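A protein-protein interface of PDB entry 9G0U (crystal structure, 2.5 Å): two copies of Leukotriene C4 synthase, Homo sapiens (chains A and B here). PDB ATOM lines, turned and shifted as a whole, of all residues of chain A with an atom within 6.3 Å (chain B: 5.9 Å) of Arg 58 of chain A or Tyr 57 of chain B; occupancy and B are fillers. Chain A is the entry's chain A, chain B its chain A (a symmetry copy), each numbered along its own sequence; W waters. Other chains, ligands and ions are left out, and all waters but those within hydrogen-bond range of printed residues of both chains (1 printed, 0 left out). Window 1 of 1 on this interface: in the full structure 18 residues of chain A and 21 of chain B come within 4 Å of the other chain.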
ATOM      1  N   PHE A  53      -2.408   7.263 -25.702  1.00  0.00           N
ATOM      2  CA  PHE A  53      -1.318   6.709 -26.502  1.00  0.00           C
ATOM      3  C   PHE A  53      -1.260   5.213 -26.211  1.00  0.00           C
ATOM      4  O   PHE A  53      -1.175   4.399 -27.140  1.00  0.00           O
ATOM      5  CB  PHE A  53       0.047   7.362 -26.135  1.00  0.00           C
ATOM      6  CG  PHE A  53       1.227   6.561 -26.643  1.00  0.00           C
ATOM      7  CD1 PHE A  53       1.639   6.660 -27.966  1.00  0.00           C
ATOM      8  CD2 PHE A  53       1.855   5.624 -25.827  1.00  0.00           C
ATOM      9  CE1 PHE A  53       2.662   5.846 -28.463  1.00  0.00           C
ATOM     10  CE2 PHE A  53       2.864   4.798 -26.329  1.00  0.00           C
ATOM     11  CZ  PHE A  53       3.272   4.927 -27.638  1.00  0.00           C
ATOM     12  N   GLU A  54      -1.298   4.861 -24.913  1.00  0.00           N
ATOM     13  CA  GLU A  54      -1.211   3.493 -24.402  1.00  0.00           C
ATOM     14  C   GLU A  54      -2.294   2.559 -24.966  1.00  0.00           C
ATOM     15  O   GLU A  54      -2.023   1.380 -25.212  1.00  0.00           O
ATOM     16  CB  GLU A  54      -1.195   3.497 -22.865  1.00  0.00           C
ATOM     17  CG  GLU A  54       0.129   3.981 -22.286  1.00  0.00           C
ATOM     18  CD  GLU A  54       0.554   3.460 -20.920  1.00  0.00           C
ATOM     19  OE1 GLU A  54      -0.178   2.634 -20.324  1.00  0.00           O
ATOM     20  OE2 GLU A  54       1.647   3.862 -20.459  1.00  0.00           O
ATOM     21  N   ARG A  55      -3.494   3.117 -25.215  1.00  0.00           N
ATOM     22  CA  ARG A  55      -4.659   2.433 -25.766  1.00  0.00           C
ATOM     23  C   ARG A  55      -4.457   2.153 -27.246  1.00  0.00           C
ATOM     24  O   ARG A  55      -4.657   1.018 -27.672  1.00  0.00           O
ATOM     25  CB  ARG A  55      -5.925   3.280 -25.547  1.00  0.00           C
ATOM     26  CG  ARG A  55      -6.528   3.147 -24.155  1.00  0.00           C
ATOM     27  CD  ARG A  55      -7.970   3.625 -24.104  1.00  0.00           C
ATOM     28  NE  ARG A  55      -8.160   4.949 -24.709  1.00  0.00           N
ATOM     29  CZ  ARG A  55      -8.022   6.106 -24.060  1.00  0.00           C
ATOM     30  NH1 ARG A  55      -8.218   7.256 -24.693  1.00  0.00           N
ATOM     31  NH2 ARG A  55      -7.678   6.121 -22.775  1.00  0.00           N
ATOM     32  N   VAL A  56      -4.052   3.187 -28.023  1.00  0.00           N
ATOM     33  CA  VAL A  56      -3.785   3.127 -29.470  1.00  0.00           C
ATOM     34  C   VAL A  56      -2.648   2.105 -29.748  1.00  0.00           C
ATOM     35  O   VAL A  56      -2.759   1.261 -30.642  1.00  0.00           O
ATOM     36  CB  VAL A  56      -3.445   4.550 -30.013  1.00  0.00           C
ATOM     37  CG1 VAL A  56      -3.140   4.531 -31.504  1.00  0.00           C
ATOM     38  CG2 VAL A  56      -4.574   5.517 -29.739  1.00  0.00           C
ATOM     39  N   TYR A  57      -1.583   2.177 -28.945  1.00  0.00           N
ATOM     40  CA  TYR A  57      -0.428   1.305 -29.020  1.00  0.00           C
ATOM     41  C   TYR A  57      -0.811  -0.151 -28.705  1.00  0.00           C
ATOM     42  O   TYR A  57      -0.340  -1.065 -29.395  1.00  0.00           O
ATOM     43  CB  TYR A  57       0.716   1.837 -28.118  1.00  0.00           C
ATOM     44  CG  TYR A  57       1.845   0.845 -27.989  1.00  0.00           C
ATOM     45  CD1 TYR A  57       2.653   0.534 -29.083  1.00  0.00           C
ATOM     46  CD2 TYR A  57       2.035   0.126 -26.813  1.00  0.00           C
ATOM     47  CE1 TYR A  57       3.627  -0.458 -29.002  1.00  0.00           C
ATOM     48  CE2 TYR A  57       2.997  -0.878 -26.727  1.00  0.00           C
ATOM     49  CZ  TYR A  57       3.802  -1.154 -27.819  1.00  0.00           C
ATOM     50  OH  TYR A  57       4.767  -2.123 -27.730  1.00  0.00           O
ATOM     51  N   ARG A  58      -1.679  -0.365 -27.695  1.00  0.00           N
ATOM     52  CA  ARG A  58      -2.134  -1.706 -27.296  1.00  0.00           C
ATOM     53  C   ARG A  58      -3.025  -2.330 -28.382  1.00  0.00           C
ATOM     54  O   ARG A  58      -2.879  -3.514 -28.683  1.00  0.00           O
ATOM     55  CB  ARG A  58      -2.815  -1.701 -25.906  1.00  0.00           C
ATOM     56  CG  ARG A  58      -3.118  -3.110 -25.386  1.00  0.00           C
ATOM     57  CD  ARG A  58      -2.210  -3.584 -24.266  1.00  0.00           C
ATOM     58  NE  ARG A  58      -0.780  -3.339 -24.494  1.00  0.00           N
ATOM     59  CZ  ARG A  58       0.053  -4.205 -25.067  1.00  0.00           C
ATOM     60  NH1 ARG A  58      -0.393  -5.386 -25.498  1.00  0.00           N
ATOM     61  NH2 ARG A  58       1.338  -3.906 -25.206  1.00  0.00           N
ATOM     62  N   ALA A  59      -3.882  -1.499 -29.009  1.00  0.00           N
ATOM     63  CA  ALA A  59      -4.784  -1.847 -30.112  1.00  0.00           C
ATOM     64  C   ALA A  59      -3.989  -2.391 -31.308  1.00  0.00           C
ATOM     65  O   ALA A  59      -4.357  -3.413 -31.884  1.00  0.00           O
ATOM     66  CB  ALA A  59      -5.594  -0.620 -30.518  1.00  0.00           C
ATOM     67  N   GLN A  60      -2.863  -1.736 -31.637  1.00  0.00           N
ATOM     68  CA  GLN A  60      -1.986  -2.121 -32.739  1.00  0.00           C
ATOM     69  C   GLN A  60      -1.276  -3.431 -32.411  1.00  0.00           C
ATOM     70  O   GLN A  60      -1.265  -4.319 -33.251  1.00  0.00           O
ATOM     71  CB  GLN A  60      -1.008  -0.990 -33.051  1.00  0.00           C
ATOM     72  CG  GLN A  60      -0.005  -1.311 -34.154  1.00  0.00           C
ATOM     73  CD  GLN A  60       1.381  -0.831 -33.821  1.00  0.00           C
ATOM     74  OE1 GLN A  60       1.897  -1.001 -32.699  1.00  0.00           O
ATOM     75  NE2 GLN A  60       2.018  -0.210 -34.797  1.00  0.00           N
ATOM     76  N   VAL A  61      -0.781  -3.586 -31.169  1.00  0.00           N
ATOM     77  CA  VAL A  61      -0.106  -4.805 -30.689  1.00  0.00           C
ATOM     78  C   VAL A  61      -1.053  -5.987 -30.787  1.00  0.00           C
ATOM     79  O   VAL A  61      -0.670  -7.017 -31.349  1.00  0.00           O
ATOM     80  CB  VAL A  61       0.537  -4.623 -29.263  1.00  0.00           C
ATOM     81  CG1 VAL A  61       0.969  -5.955 -28.645  1.00  0.00           C
ATOM     82  CG2 VAL A  61       1.715  -3.677 -29.329  1.00  0.00           C
ATOM     83  N   ASN A  62      -2.320  -5.800 -30.331  1.00  0.00           N
ATOM     84  CA  ASN A  62      -3.363  -6.831 -30.362  1.00  0.00           C
ATOM     85  C   ASN A  62      -3.704  -7.268 -31.767  1.00  0.00           C
ATOM     86  O   ASN A  62      -3.724  -8.466 -32.027  1.00  0.00           O
ATOM     87  CB  ASN A  62      -4.595  -6.394 -29.591  1.00  0.00           C
ATOM     88  CG  ASN A  62      -4.335  -6.240 -28.128  1.00  0.00           C
ATOM     89  OD1 ASN A  62      -3.582  -6.988 -27.535  1.00  0.00           O
ATOM     90  ND2 ASN A  62      -4.948  -5.256 -27.513  1.00  0.00           N
ATOM     91  N   CYS A  63      -3.899  -6.304 -32.690  1.00  0.00           N
ATOM     92  CA  CYS A  63      -4.155  -6.544 -34.111  1.00  0.00           C
ATOM     93  C   CYS A  63      -2.980  -7.259 -34.779  1.00  0.00           C
ATOM     94  O   CYS A  63      -3.189  -8.122 -35.614  1.00  0.00           O
ATOM     95  CB  CYS A  63      -4.506  -5.247 -34.825  1.00  0.00           C
ATOM     96  SG  CYS A  63      -6.117  -4.556 -34.358  1.00  0.00           S
ATOM     97  N   GLU A  65      -0.783  -9.319 -33.062  1.00  0.00           N
ATOM     98  CA  GLU A  65      -0.761 -10.689 -32.546  1.00  0.00           C
ATOM     99  C   GLU A  65      -1.689 -11.622 -33.346  1.00  0.00           C
ATOM    100  O   GLU A  65      -1.328 -12.761 -33.646  1.00  0.00           O
ATOM    101  CB  GLU A  65      -1.205 -10.727 -31.079  1.00  0.00           C
ATOM    102  CG  GLU A  65      -0.259 -10.031 -30.126  1.00  0.00           C
ATOM    103  CD  GLU A  65      -0.023 -10.719 -28.794  1.00  0.00           C
ATOM    104  OE1 GLU A  65      -0.783 -11.657 -28.442  1.00  0.00           O
ATOM    105  OE2 GLU A  65       0.964 -10.332 -28.121  1.00  0.00           O
ATOM    106  N   TYR A 100     -12.598  -1.729 -33.850  1.00  0.00           N
ATOM    107  CA  TYR A 100     -11.960  -2.080 -32.576  1.00  0.00           C
ATOM    108  C   TYR A 100     -10.891  -1.023 -32.280  1.00  0.00           C
ATOM    109  O   TYR A 100     -10.838  -0.453 -31.177  1.00  0.00           O
ATOM    110  CB  TYR A 100     -11.319  -3.498 -32.695  1.00  0.00           C
ATOM    111  CG  TYR A 100     -10.268  -3.807 -31.644  1.00  0.00           C
ATOM    112  CD1 TYR A 100     -10.632  -4.090 -30.327  1.00  0.00           C
ATOM    113  CD2 TYR A 100      -8.910  -3.790 -31.958  1.00  0.00           C
ATOM    114  CE1 TYR A 100      -9.670  -4.353 -29.353  1.00  0.00           C
ATOM    115  CE2 TYR A 100      -7.941  -4.057 -30.989  1.00  0.00           C
ATOM    116  CZ  TYR A 100      -8.331  -4.359 -29.696  1.00  0.00           C
ATOM    117  OH  TYR A 100      -7.405  -4.635 -28.729  1.00  0.00           O
ATOM    118  N   TYR A 104     -11.136   1.594 -29.287  1.00  0.00           N
ATOM    119  CA  TYR A 104     -10.062   1.524 -28.287  1.00  0.00           C
ATOM    120  C   TYR A 104      -9.309   2.842 -28.156  1.00  0.00           C
ATOM    121  O   TYR A 104      -8.979   3.220 -27.038  1.00  0.00           O
ATOM    122  CB  TYR A 104      -9.085   0.391 -28.643  1.00  0.00           C
ATOM    123  CG  TYR A 104      -8.373  -0.277 -27.481  1.00  0.00           C
ATOM    124  CD1 TYR A 104      -8.365   0.299 -26.212  1.00  0.00           C
ATOM    125  CD2 TYR A 104      -7.623  -1.434 -27.675  1.00  0.00           C
ATOM    126  CE1 TYR A 104      -7.691  -0.300 -25.151  1.00  0.00           C
ATOM    127  CE2 TYR A 104      -6.947  -2.042 -26.620  1.00  0.00           C
ATOM    128  CZ  TYR A 104      -6.999  -1.482 -25.355  1.00  0.00           C
ATOM    129  OH  TYR A 104      -6.348  -2.086 -24.314  1.00  0.00           O
ATOM    130  N   VAL B  33      -4.565 -15.861 -20.199  1.00  0.00           N
ATOM    131  CA  VAL B  33      -4.201 -14.477 -19.908  1.00  0.00           C
ATOM    132  C   VAL B  33      -5.462 -13.670 -19.481  1.00  0.00           C
ATOM    133  O   VAL B  33      -5.378 -12.887 -18.537  1.00  0.00           O
ATOM    134  CB  VAL B  33      -3.422 -13.820 -21.069  1.00  0.00           C
ATOM    135  CG1 VAL B  33      -3.077 -12.362 -20.735  1.00  0.00           C
ATOM    136  CG2 VAL B  33      -2.158 -14.615 -21.381  1.00  0.00           C
ATOM    137  N   ARG B  37      -5.938 -11.886 -15.892  1.00  0.00           N
ATOM    138  CA  ARG B  37      -6.401 -10.501 -15.889  1.00  0.00           C
ATOM    139  C   ARG B  37      -7.481 -10.245 -14.852  1.00  0.00           C
ATOM    140  O   ARG B  37      -7.473  -9.169 -14.263  1.00  0.00           O
ATOM    141  CB  ARG B  37      -6.824 -10.046 -17.283  1.00  0.00           C
ATOM    142  CG  ARG B  37      -5.626  -9.623 -18.087  1.00  0.00           C
ATOM    143  CD  ARG B  37      -5.968  -8.778 -19.287  1.00  0.00           C
ATOM    144  NE  ARG B  37      -4.730  -8.387 -19.955  1.00  0.00           N
ATOM    145  CZ  ARG B  37      -4.176  -7.183 -19.878  1.00  0.00           C
ATOM    146  NH1 ARG B  37      -3.032  -6.935 -20.500  1.00  0.00           N
ATOM    147  NH2 ARG B  37      -4.778  -6.210 -19.209  1.00  0.00           N
ATOM    148  N   PRO B  45      -5.593  -0.767 -20.423  1.00  0.00           N
ATOM    149  CA  PRO B  45      -4.587  -1.149 -21.384  1.00  0.00           C
ATOM    150  C   PRO B  45      -3.259  -1.562 -20.760  1.00  0.00           C
ATOM    151  O   PRO B  45      -2.256  -1.360 -21.373  1.00  0.00           O
ATOM    152  CB  PRO B  45      -4.368   0.220 -22.018  1.00  0.00           C
ATOM    153  CG  PRO B  45      -4.392   1.180 -20.862  1.00  0.00           C
ATOM    154  CD  PRO B  45      -5.345   0.559 -19.867  1.00  0.00           C
ATOM    155  N   LEU B  46      -3.292  -2.205 -19.603  1.00  0.00           N
ATOM    156  CA  LEU B  46      -2.017  -2.464 -18.896  1.00  0.00           C
ATOM    157  C   LEU B  46      -1.524  -3.898 -19.064  1.00  0.00           C
ATOM    158  O   LEU B  46      -2.359  -4.792 -19.140  1.00  0.00           O
ATOM    159  CB  LEU B  46      -2.224  -2.109 -17.422  1.00  0.00           C
ATOM    160  CG  LEU B  46      -2.805  -0.724 -17.154  1.00  0.00           C
ATOM    161  CD1 LEU B  46      -3.234  -0.596 -15.703  1.00  0.00           C
ATOM    162  CD2 LEU B  46      -1.804   0.360 -17.511  1.00  0.00           C
ATOM    163  N   THR B  47      -0.204  -4.082 -19.055  1.00  0.00           N
ATOM    164  CA  THR B  47       0.438  -5.404 -19.254  1.00  0.00           C
ATOM    165  C   THR B  47       1.339  -5.710 -18.061  1.00  0.00           C
ATOM    166  O   THR B  47       1.934  -6.785 -18.039  1.00  0.00           O
ATOM    167  CB  THR B  47       1.297  -5.374 -20.521  1.00  0.00           C
ATOM    168  OG1 THR B  47       2.424  -4.528 -20.308  1.00  0.00           O
ATOM    169  CG2 THR B  47       0.532  -4.903 -21.737  1.00  0.00           C
ATOM    170  N   GLU B  52       3.412 -13.475 -11.304  1.00  0.00           N
ATOM    171  CA  GLU B  52       2.662 -14.613 -11.862  1.00  0.00           C
ATOM    172  C   GLU B  52       1.917 -14.229 -13.132  1.00  0.00           C
ATOM    173  O   GLU B  52       2.009 -14.955 -14.124  1.00  0.00           O
ATOM    174  CB  GLU B  52       1.704 -15.211 -10.821  1.00  0.00           C
ATOM    175  CG  GLU B  52       0.554 -16.054 -11.365  1.00  0.00           C
ATOM    176  CD  GLU B  52       0.809 -17.509 -11.705  1.00  0.00           C
ATOM    177  OE1 GLU B  52       0.390 -17.930 -12.809  1.00  0.00           O
ATOM    178  OE2 GLU B  52       1.348 -18.246 -10.845  1.00  0.00           O
ATOM    179  N   PHE B  53       1.177 -13.101 -13.099  1.00  0.00           N
ATOM    180  CA  PHE B  53       0.458 -12.557 -14.249  1.00  0.00           C
ATOM    181  C   PHE B  53       1.494 -12.263 -15.330  1.00  0.00           C
ATOM    182  O   PHE B  53       1.298 -12.625 -16.497  1.00  0.00           O
ATOM    183  CB  PHE B  53      -0.296 -11.246 -13.881  1.00  0.00           C
ATOM    184  CG  PHE B  53      -0.716 -10.458 -15.104  1.00  0.00           C
ATOM    185  CD1 PHE B  53      -1.855 -10.806 -15.819  1.00  0.00           C
ATOM    186  CD2 PHE B  53       0.090  -9.439 -15.605  1.00  0.00           C
ATOM    187  CE1 PHE B  53      -2.188 -10.144 -17.006  1.00  0.00           C
ATOM    188  CE2 PHE B  53      -0.234  -8.792 -16.801  1.00  0.00           C
ATOM    189  CZ  PHE B  53      -1.379  -9.137 -17.483  1.00  0.00           C
ATOM    190  N   GLU B  54       2.591 -11.594 -14.930  1.00  0.00           N
ATOM    191  CA  GLU B  54       3.687 -11.167 -15.800  1.00  0.00           C
ATOM    192  C   GLU B  54       4.342 -12.325 -16.572  1.00  0.00           C
ATOM    193  O   GLU B  54       4.734 -12.149 -17.730  1.00  0.00           O
ATOM    194  CB  GLU B  54       4.716 -10.351 -15.002  1.00  0.00           C
ATOM    195  CG  GLU B  54       4.222  -8.953 -14.651  1.00  0.00           C
ATOM    196  CD  GLU B  54       5.250  -7.846 -14.474  1.00  0.00           C
ATOM    197  OE1 GLU B  54       6.466  -8.104 -14.645  1.00  0.00           O
ATOM    198  OE2 GLU B  54       4.829  -6.700 -14.191  1.00  0.00           O
ATOM    199  N   ARG B  55       4.401 -13.510 -15.936  1.00  0.00           N
ATOM    200  CA  ARG B  55       4.958 -14.746 -16.476  1.00  0.00           C
ATOM    201  C   ARG B  55       4.028 -15.330 -17.526  1.00  0.00           C
ATOM    202  O   ARG B  55       4.488 -15.652 -18.620  1.00  0.00           O
ATOM    203  CB  ARG B  55       5.195 -15.761 -15.344  1.00  0.00           C
ATOM    204  CG  ARG B  55       6.488 -15.538 -14.571  1.00  0.00           C
ATOM    205  CD  ARG B  55       6.906 -16.767 -13.781  1.00  0.00           C
ATOM    206  NE  ARG B  55       5.819 -17.327 -12.969  1.00  0.00           N
ATOM    207  CZ  ARG B  55       5.525 -16.944 -11.726  1.00  0.00           C
ATOM    208  NH1 ARG B  55       4.522 -17.513 -11.069  1.00  0.00           N
ATOM    209  NH2 ARG B  55       6.227 -15.980 -11.135  1.00  0.00           N
ATOM    210  N   VAL B  56       2.720 -15.456 -17.195  1.00  0.00           N
ATOM    211  CA  VAL B  56       1.655 -15.982 -18.065  1.00  0.00           C
ATOM    212  C   VAL B  56       1.538 -15.097 -19.337  1.00  0.00           C
ATOM    213  O   VAL B  56       1.472 -15.606 -20.460  1.00  0.00           O
ATOM    214  CB  VAL B  56       0.309 -16.065 -17.279  1.00  0.00           C
ATOM    215  CG1 VAL B  56      -0.826 -16.584 -18.150  1.00  0.00           C
ATOM    216  CG2 VAL B  56       0.452 -16.943 -16.056  1.00  0.00           C
ATOM    217  N   TYR B  57       1.551 -13.776 -19.138  1.00  0.00           N
ATOM    218  CA  TYR B  57       1.475 -12.778 -20.186  1.00  0.00           C
ATOM    219  C   TYR B  57       2.706 -12.849 -21.107  1.00  0.00           C
ATOM    220  O   TYR B  57       2.552 -12.751 -22.333  1.00  0.00           O
ATOM    221  CB  TYR B  57       1.254 -11.368 -19.582  1.00  0.00           C
ATOM    222  CG  TYR B  57       1.397 -10.278 -20.615  1.00  0.00           C
ATOM    223  CD1 TYR B  57       0.469 -10.144 -21.647  1.00  0.00           C
ATOM    224  CD2 TYR B  57       2.521  -9.457 -20.637  1.00  0.00           C
ATOM    225  CE1 TYR B  57       0.652  -9.211 -22.665  1.00  0.00           C
ATOM    226  CE2 TYR B  57       2.719  -8.531 -21.659  1.00  0.00           C
ATOM    227  CZ  TYR B  57       1.773  -8.400 -22.661  1.00  0.00           C
ATOM    228  OH  TYR B  57       1.951  -7.473 -23.654  1.00  0.00           O
ATOM    229  N   ARG B  58       3.908 -13.045 -20.530  1.00  0.00           N
ATOM    230  CA  ARG B  58       5.162 -13.139 -21.295  1.00  0.00           C
ATOM    231  C   ARG B  58       5.197 -14.425 -22.137  1.00  0.00           C
ATOM    232  O   ARG B  58       5.612 -14.385 -23.294  1.00  0.00           O
ATOM    233  CB  ARG B  58       6.410 -12.993 -20.391  1.00  0.00           C
ATOM    234  CG  ARG B  58       7.714 -12.890 -21.188  1.00  0.00           C
ATOM    235  CD  ARG B  58       8.329 -11.503 -21.227  1.00  0.00           C
ATOM    236  NE  ARG B  58       7.379 -10.422 -21.518  1.00  0.00           N
ATOM    237  CZ  ARG B  58       7.111  -9.959 -22.737  1.00  0.00           C
ATOM    238  NH1 ARG B  58       7.707 -10.490 -23.806  1.00  0.00           N
ATOM    239  NH2 ARG B  58       6.257  -8.958 -22.899  1.00  0.00           N
ATOM    240  N   ALA B  59       4.686 -15.534 -21.564  1.00  0.00           N
ATOM    241  CA  ALA B  59       4.555 -16.855 -22.186  1.00  0.00           C
ATOM    242  C   ALA B  59       3.698 -16.771 -23.457  1.00  0.00           C
ATOM    243  O   ALA B  59       4.068 -17.321 -24.493  1.00  0.00           O
ATOM    244  CB  ALA B  59       3.941 -17.833 -21.189  1.00  0.00           C
ATOM    245  N   GLN B  60       2.581 -16.026 -23.389  1.00  0.00           N
ATOM    246  CA  GLN B  60       1.658 -15.832 -24.504  1.00  0.00           C
ATOM    247  C   GLN B  60       2.313 -14.975 -25.583  1.00  0.00           C
ATOM    248  O   GLN B  60       2.253 -15.350 -26.745  1.00  0.00           O
ATOM    249  CB  GLN B  60       0.346 -15.235 -24.000  1.00  0.00           C
ATOM    250  CG  GLN B  60      -0.673 -14.939 -25.095  1.00  0.00           C
ATOM    251  CD  GLN B  60      -1.360 -13.616 -24.892  1.00  0.00           C
ATOM    252  OE1 GLN B  60      -0.740 -12.580 -24.581  1.00  0.00           O
ATOM    253  NE2 GLN B  60      -2.670 -13.623 -25.061  1.00  0.00           N
ATOM    254  N   VAL B  61       3.014 -13.895 -25.191  1.00  0.00           N
ATOM    255  CA  VAL B  61       3.734 -12.995 -26.109  1.00  0.00           C
ATOM    256  C   VAL B  61       4.785 -13.777 -26.875  1.00  0.00           C
ATOM    257  O   VAL B  61       4.826 -13.680 -28.105  1.00  0.00           O
ATOM    258  CB  VAL B  61       4.297 -11.714 -25.385  1.00  0.00           C
ATOM    259  CG1 VAL B  61       5.287 -10.940 -26.260  1.00  0.00           C
ATOM    260  CG2 VAL B  61       3.167 -10.806 -24.957  1.00  0.00           C
ATOM    261  N   ASN B  62       5.565 -14.627 -26.156  1.00  0.00           N
ATOM    262  CA  ASN B  62       6.618 -15.466 -26.740  1.00  0.00           C
ATOM    263  C   ASN B  62       6.077 -16.463 -27.738  1.00  0.00           C
ATOM    264  O   ASN B  62       6.604 -16.541 -28.842  1.00  0.00           O
ATOM    265  CB  ASN B  62       7.449 -16.138 -25.663  1.00  0.00           C
ATOM    266  CG  ASN B  62       8.230 -15.162 -24.844  1.00  0.00           C
ATOM    267  OD1 ASN B  62       8.717 -14.165 -25.340  1.00  0.00           O
ATOM    268  ND2 ASN B  62       8.356 -15.424 -23.564  1.00  0.00           N
ATOM    269  N   PHE B 101       4.179 -23.079 -21.579  1.00  0.00           N
ATOM    270  CA  PHE B 101       3.190 -22.156 -21.063  1.00  0.00           C
ATOM    271  C   PHE B 101       2.805 -22.494 -19.629  1.00  0.00           C
ATOM    272  O   PHE B 101       2.864 -21.630 -18.750  1.00  0.00           O
ATOM    273  CB  PHE B 101       1.982 -22.092 -22.006  1.00  0.00           C
ATOM    274  CG  PHE B 101       1.036 -20.964 -21.669  1.00  0.00           C
ATOM    275  CD1 PHE B 101       0.041 -21.129 -20.701  1.00  0.00           C
ATOM    276  CD2 PHE B 101       1.144 -19.733 -22.304  1.00  0.00           C
ATOM    277  CE1 PHE B 101      -0.816 -20.076 -20.372  1.00  0.00           C
ATOM    278  CE2 PHE B 101       0.283 -18.681 -21.969  1.00  0.00           C
ATOM    279  CZ  PHE B 101      -0.683 -18.854 -20.998  1.00  0.00           C
HETATM  280  O   HOH W   1       3.938 -11.271 -29.644  1.00  0.00           O
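Among the printed residues, merely in contact across the chains: Arg 58 of chain A with Thr 47 of chain B, Tyr 104 of chain A with Pro 45 of chain B, Arg 58 of chain A with Tyr 57 of chain B, Arg 58 of chain A with Pro 45 of chain B, Glu 65 of chain A with Val 61 of chain B, Glu 54 of chain A with Leu 46 of chain B and Glu 65 of chain A with Gln 60 of chain B.
Printed residues of chain A that touch a printed residue of chain B: Glu 54, Arg 58, Glu 65 and Tyr 104.
Hydrophobic or aromatic side chains of chain A within 4 Å of the printed part of chain B: Tyr 104.
Hydrophobic or aromatic side chains of chain B that line the printed part of chain A: Pro 45, Leu 46, Tyr 57 and Val 61.
O of Leu 46 of chain B sits at hydrogen-bond distance from NH1 of Arg 37 of chain B, at 2.6 Å.
NE of Arg 55 of chain A lies within hydrogen-bond range of O of Tyr 104 of chain A (3.0 Å).
The backbone carbonyl oxygen (O) of Arg 58 of chain A is in hydrogen-bond range of the side-chain amide nitrogen (ND2) of Asn 62 of chain A, at 2.9 Å.
Water W1 bridges O of Val 61 of chain B and OE2 of Glu 65 of chain A.
Tyr 57 of chain B touches just one residue of chain A: Arg 58 (3.6 Å).
Of the printed residues of chain B, Glu 65 of chain A touches Gln 60 (3.97 Å) and Val 61 (3.9 Å).
Of the printed residues of chain B, Tyr 104 of chain A touches Pro 45 (3.5 Å).
Of the printed residues of chain A, Thr 47 of chain B touches Arg 58 (3.4 Å).
Of the printed residues of chain B, Glu 54 of chain A touches Leu 46.
Arg 55 of chain B touches none of the printed residues of chain A.
The nearest residue of chain B that does not touch Arg 58 of chain A is Leu 46 of chain B (5.0 Å).
The nearest residue of chain A that does not touch Tyr 57 of chain B is Val 61 of chain A (5.3 Å).
Arg 58 of chain A touches Tyr 57 of chain B, but with the chains exchanged Tyr 57 of chain A does not touch Arg 58 of chain B (8.5 Å).
10 positions are printed for both chains.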
